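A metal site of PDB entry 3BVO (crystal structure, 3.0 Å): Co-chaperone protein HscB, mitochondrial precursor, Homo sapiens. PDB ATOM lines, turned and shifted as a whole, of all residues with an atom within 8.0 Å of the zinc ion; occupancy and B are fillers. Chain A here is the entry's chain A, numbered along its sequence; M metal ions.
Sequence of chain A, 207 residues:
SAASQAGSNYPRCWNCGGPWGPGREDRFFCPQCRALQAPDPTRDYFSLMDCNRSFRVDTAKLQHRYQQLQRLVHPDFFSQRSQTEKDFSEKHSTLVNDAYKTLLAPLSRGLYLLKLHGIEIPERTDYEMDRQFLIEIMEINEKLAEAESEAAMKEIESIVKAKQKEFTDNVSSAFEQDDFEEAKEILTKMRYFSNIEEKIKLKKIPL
The zinc ion is bound by SG of Cys 30, at 2.3 Å.
The zinc ion is bound by SG of Cys 33, at 2.3 Å.
The zinc ion is bound by SG of Cys 13 (2.3 Å).
The zinc ion is bound by SG of Cys 16.
The side-chain sulfur (SG) of Cys 30 sits close to the backbone NH (N) of Gln 32, 3.2 Å away.
O of Ala 35 sits at hydrogen-bond distance from N of Cys 30.
The side-chain sulfur of Cys 33 sits close to the backbone NH of Ala 35, 3.8 Å away.
The side-chain sulfur (SG) of Cys 13 lies close to the backbone NH (N) of Asn 15 (3.1 Å).
SG of Cys 13 sits close to NE2 of Gln 37 (3.8 Å).
N of Cys 13 is in hydrogen-bond range of O of Gly 18 (2.9 Å).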
ATOM      1  N   ARG A  12      20.313  23.608  13.127  1.00  0.00           N
ATOM      2  CA  ARG A  12      20.005  23.112  14.464  1.00  0.00           C
ATOM      3  C   ARG A  12      18.844  23.900  15.059  1.00  0.00           C
ATOM      4  O   ARG A  12      18.551  24.999  14.602  1.00  0.00           O
ATOM      5  CB  ARG A  12      21.227  23.247  15.378  1.00  0.00           C
ATOM      6  CG  ARG A  12      21.663  24.688  15.623  1.00  0.00           C
ATOM      7  CD  ARG A  12      23.133  24.773  15.989  1.00  0.00           C
ATOM      8  NE  ARG A  12      23.982  24.387  14.864  1.00  0.00           N
ATOM      9  CZ  ARG A  12      24.650  23.242  14.772  1.00  0.00           C
ATOM     10  NH1 ARG A  12      25.388  22.997  13.696  1.00  0.00           N
ATOM     11  NH2 ARG A  12      24.596  22.334  15.741  1.00  0.00           N
ATOM     12  N   CYS A  13      18.213  23.354  16.087  1.00  0.00           N
ATOM     13  CA  CYS A  13      17.013  23.963  16.649  1.00  0.00           C
ATOM     14  C   CYS A  13      17.351  25.083  17.617  1.00  0.00           C
ATOM     15  O   CYS A  13      18.257  24.944  18.429  1.00  0.00           O
ATOM     16  CB  CYS A  13      16.158  22.920  17.345  1.00  0.00           C
ATOM     17  SG  CYS A  13      14.944  23.654  18.430  1.00  0.00           S
ATOM     18  N   TRP A  14      16.604  26.180  17.558  1.00  0.00           N
ATOM     19  CA  TRP A  14      16.868  27.359  18.378  1.00  0.00           C
ATOM     20  C   TRP A  14      16.525  27.144  19.852  1.00  0.00           C
ATOM     21  O   TRP A  14      16.987  27.898  20.713  1.00  0.00           O
ATOM     22  CB  TRP A  14      16.139  28.601  17.841  1.00  0.00           C
ATOM     23  CG  TRP A  14      14.649  28.550  17.968  1.00  0.00           C
ATOM     24  CD1 TRP A  14      13.743  28.113  17.018  1.00  0.00           C
ATOM     25  CD2 TRP A  14      13.863  28.967  19.096  1.00  0.00           C
ATOM     26  NE1 TRP A  14      12.454  28.228  17.492  1.00  0.00           N
ATOM     27  CE2 TRP A  14      12.493  28.739  18.765  1.00  0.00           C
ATOM     28  CE3 TRP A  14      14.175  29.498  20.361  1.00  0.00           C
ATOM     29  CZ2 TRP A  14      11.450  29.046  19.652  1.00  0.00           C
ATOM     30  CZ3 TRP A  14      13.145  29.802  21.240  1.00  0.00           C
ATOM     31  CH2 TRP A  14      11.789  29.577  20.876  1.00  0.00           C
ATOM     32  N   ASN A  15      15.754  26.094  20.137  1.00  0.00           N
ATOM     33  CA  ASN A  15      15.390  25.741  21.507  1.00  0.00           C
ATOM     34  C   ASN A  15      16.245  24.610  22.081  1.00  0.00           C
ATOM     35  O   ASN A  15      16.794  24.758  23.168  1.00  0.00           O
ATOM     36  CB  ASN A  15      13.910  25.400  21.609  1.00  0.00           C
ATOM     37  CG  ASN A  15      13.295  25.865  22.926  1.00  0.00           C
ATOM     38  OD1 ASN A  15      13.900  26.626  23.672  1.00  0.00           O
ATOM     39  ND2 ASN A  15      12.081  25.394  23.209  1.00  0.00           N
ATOM     40  N   CYS A  16      16.334  23.481  21.365  1.00  0.00           N
ATOM     41  CA  CYS A  16      17.103  22.311  21.816  1.00  0.00           C
ATOM     42  C   CYS A  16      18.554  22.396  21.433  1.00  0.00           C
ATOM     43  O   CYS A  16      19.444  22.152  22.248  1.00  0.00           O
ATOM     44  CB  CYS A  16      16.611  21.018  21.152  1.00  0.00           C
ATOM     45  SG  CYS A  16      14.896  20.654  21.164  1.00  0.00           S
ATOM     46  N   GLY A  17      18.801  22.708  20.161  1.00  0.00           N
ATOM     47  CA  GLY A  17      20.071  22.406  19.540  1.00  0.00           C
ATOM     48  C   GLY A  17      19.933  21.080  18.808  1.00  0.00           C
ATOM     49  O   GLY A  17      20.928  20.537  18.310  1.00  0.00           O
ATOM     50  N   GLY A  18      18.705  20.581  18.747  1.00  0.00           N
ATOM     51  CA  GLY A  18      18.383  19.343  18.035  1.00  0.00           C
ATOM     52  C   GLY A  18      18.737  19.462  16.568  1.00  0.00           C
ATOM     53  O   GLY A  18      18.385  20.441  15.927  1.00  0.00           O
ATOM     54  N   PRO A  19      19.460  18.464  16.037  1.00  0.00           N
ATOM     55  CA  PRO A  19      19.955  18.539  14.669  1.00  0.00           C
ATOM     56  C   PRO A  19      18.822  18.436  13.653  1.00  0.00           C
ATOM     57  O   PRO A  19      17.929  17.602  13.805  1.00  0.00           O
ATOM     58  CB  PRO A  19      20.866  17.321  14.557  1.00  0.00           C
ATOM     59  CG  PRO A  19      21.116  16.880  15.974  1.00  0.00           C
ATOM     60  CD  PRO A  19      19.866  17.208  16.687  1.00  0.00           C
ATOM     61  N   TRP A  20      18.854  19.303  12.640  1.00  0.00           N
ATOM     62  CA  TRP A  20      17.975  19.209  11.475  1.00  0.00           C
ATOM     63  C   TRP A  20      18.395  18.014  10.641  1.00  0.00           C
ATOM     64  O   TRP A  20      19.509  18.002  10.090  1.00  0.00           O
ATOM     65  CB  TRP A  20      18.094  20.462  10.612  1.00  0.00           C
ATOM     66  CG  TRP A  20      17.248  21.612  11.028  1.00  0.00           C
ATOM     67  CD1 TRP A  20      16.880  21.938  12.307  1.00  0.00           C
ATOM     68  CD2 TRP A  20      16.683  22.613  10.185  1.00  0.00           C
ATOM     69  NE1 TRP A  20      16.101  23.078  12.296  1.00  0.00           N
ATOM     70  CE2 TRP A  20      15.972  23.518  11.004  1.00  0.00           C
ATOM     71  CE3 TRP A  20      16.708  22.842   8.794  1.00  0.00           C
ATOM     72  CZ2 TRP A  20      15.289  24.621  10.492  1.00  0.00           C
ATOM     73  CZ3 TRP A  20      16.017  23.935   8.286  1.00  0.00           C
ATOM     74  CH2 TRP A  20      15.321  24.818   9.138  1.00  0.00           C
ATOM     75  N   PHE A  29       8.196  22.083  12.495  1.00  0.00           N
ATOM     76  CA  PHE A  29       8.279  21.919  13.935  1.00  0.00           C
ATOM     77  C   PHE A  29       9.386  20.987  14.355  1.00  0.00           C
ATOM     78  O   PHE A  29       9.682  20.015  13.675  1.00  0.00           O
ATOM     79  CB  PHE A  29       6.948  21.432  14.479  1.00  0.00           C
ATOM     80  CG  PHE A  29       5.840  22.396  14.280  1.00  0.00           C
ATOM     81  CD1 PHE A  29       5.736  23.530  15.090  1.00  0.00           C
ATOM     82  CD2 PHE A  29       4.906  22.215  13.270  1.00  0.00           C
ATOM     83  CE1 PHE A  29       4.702  24.459  14.906  1.00  0.00           C
ATOM     84  CE2 PHE A  29       3.871  23.123  13.075  1.00  0.00           C
ATOM     85  CZ  PHE A  29       3.769  24.249  13.890  1.00  0.00           C
ATOM     86  N   CYS A  30      10.006  21.307  15.490  1.00  0.00           N
ATOM     87  CA  CYS A  30      11.066  20.486  16.032  1.00  0.00           C
ATOM     88  C   CYS A  30      10.509  19.178  16.581  1.00  0.00           C
ATOM     89  O   CYS A  30       9.658  19.193  17.451  1.00  0.00           O
ATOM     90  CB  CYS A  30      11.759  21.239  17.151  1.00  0.00           C
ATOM     91  SG  CYS A  30      12.922  20.247  18.069  1.00  0.00           S
ATOM     92  N   PRO A  31      10.979  18.045  16.056  1.00  0.00           N
ATOM     93  CA  PRO A  31      10.439  16.793  16.574  1.00  0.00           C
ATOM     94  C   PRO A  31      10.731  16.564  18.065  1.00  0.00           C
ATOM     95  O   PRO A  31      10.080  15.727  18.698  1.00  0.00           O
ATOM     96  CB  PRO A  31      11.121  15.716  15.710  1.00  0.00           C
ATOM     97  CG  PRO A  31      12.278  16.361  15.090  1.00  0.00           C
ATOM     98  CD  PRO A  31      11.947  17.820  14.968  1.00  0.00           C
ATOM     99  N   GLN A  32      11.694  17.312  18.603  1.00  0.00           N
ATOM    100  CA  GLN A  32      12.210  17.057  19.944  1.00  0.00           C
ATOM    101  C   GLN A  32      11.546  17.919  20.990  1.00  0.00           C
ATOM    102  O   GLN A  32      11.423  17.495  22.133  1.00  0.00           O
ATOM    103  CB  GLN A  32      13.722  17.276  19.991  1.00  0.00           C
ATOM    104  CG  GLN A  32      14.526  16.348  19.097  1.00  0.00           C
ATOM    105  CD  GLN A  32      16.019  16.369  19.390  1.00  0.00           C
ATOM    106  OE1 GLN A  32      16.491  17.136  20.233  1.00  0.00           O
ATOM    107  NE2 GLN A  32      16.767  15.514  18.705  1.00  0.00           N
ATOM    108  N   CYS A  33      11.129  19.130  20.598  1.00  0.00           N
ATOM    109  CA  CYS A  33      10.585  20.119  21.539  1.00  0.00           C
ATOM    110  C   CYS A  33       9.302  20.850  21.050  1.00  0.00           C
ATOM    111  O   CYS A  33       8.731  21.665  21.794  1.00  0.00           O
ATOM    112  CB  CYS A  33      11.668  21.119  21.949  1.00  0.00           C
ATOM    113  SG  CYS A  33      12.062  22.358  20.705  1.00  0.00           S
ATOM    114  N   ARG A  34       8.877  20.561  19.828  1.00  0.00           N
ATOM    115  CA  ARG A  34       7.622  21.039  19.257  1.00  0.00           C
ATOM    116  C   ARG A  34       7.641  22.527  18.869  1.00  0.00           C
ATOM    117  O   ARG A  34       6.630  23.062  18.393  1.00  0.00           O
ATOM    118  CB  ARG A  34       6.440  20.725  20.187  1.00  0.00           C
ATOM    119  CG  ARG A  34       5.148  20.338  19.486  1.00  0.00           C
ATOM    120  CD  ARG A  34       4.086  20.011  20.511  1.00  0.00           C
ATOM    121  NE  ARG A  34       2.746  20.322  20.048  1.00  0.00           N
ATOM    122  CZ  ARG A  34       1.710  19.487  20.080  1.00  0.00           C
ATOM    123  NH1 ARG A  34       1.838  18.269  20.568  1.00  0.00           N
ATOM    124  NH2 ARG A  34       0.525  19.879  19.608  1.00  0.00           N
ATOM    125  N   ALA A  35       8.785  23.186  19.041  1.00  0.00           N
ATOM    126  CA  ALA A  35       8.960  24.603  18.713  1.00  0.00           C
ATOM    127  C   ALA A  35       8.928  24.886  17.210  1.00  0.00           C
ATOM    128  O   ALA A  35       9.392  24.070  16.399  1.00  0.00           O
ATOM    129  CB  ALA A  35      10.256  25.112  19.306  1.00  0.00           C
ATOM    130  N   LEU A  36       8.363  26.034  16.816  1.00  0.00           N
ATOM    131  CA  LEU A  36       8.277  26.398  15.415  1.00  0.00           C
ATOM    132  C   LEU A  36       9.626  26.887  14.967  1.00  0.00           C
ATOM    133  O   LEU A  36      10.207  27.771  15.579  1.00  0.00           O
ATOM    134  CB  LEU A  36       7.222  27.491  15.199  1.00  0.00           C
ATOM    135  CG  LEU A  36       6.984  27.920  13.731  1.00  0.00           C
ATOM    136  CD1 LEU A  36       5.833  27.165  13.111  1.00  0.00           C
ATOM    137  CD2 LEU A  36       6.721  29.397  13.611  1.00  0.00           C
ATOM    138  N   GLN A  37      10.126  26.318  13.882  1.00  0.00           N
ATOM    139  CA  GLN A  37      11.494  26.570  13.440  1.00  0.00           C
ATOM    140  C   GLN A  37      11.586  27.777  12.509  1.00  0.00           C
ATOM    141  O   GLN A  37      10.578  28.196  11.935  1.00  0.00           O
ATOM    142  CB  GLN A  37      12.069  25.332  12.748  1.00  0.00           C
ATOM    143  CG  GLN A  37      11.968  24.076  13.570  1.00  0.00           C
ATOM    144  CD  GLN A  37      12.805  24.157  14.829  1.00  0.00           C
ATOM    145  OE1 GLN A  37      14.028  24.062  14.763  1.00  0.00           O
ATOM    146  NE2 GLN A  37      12.150  24.326  15.964  1.00  0.00           N
HETATM  147 ZN    ZN M   1      13.917  21.830  19.422  1.00  0.00          ZN
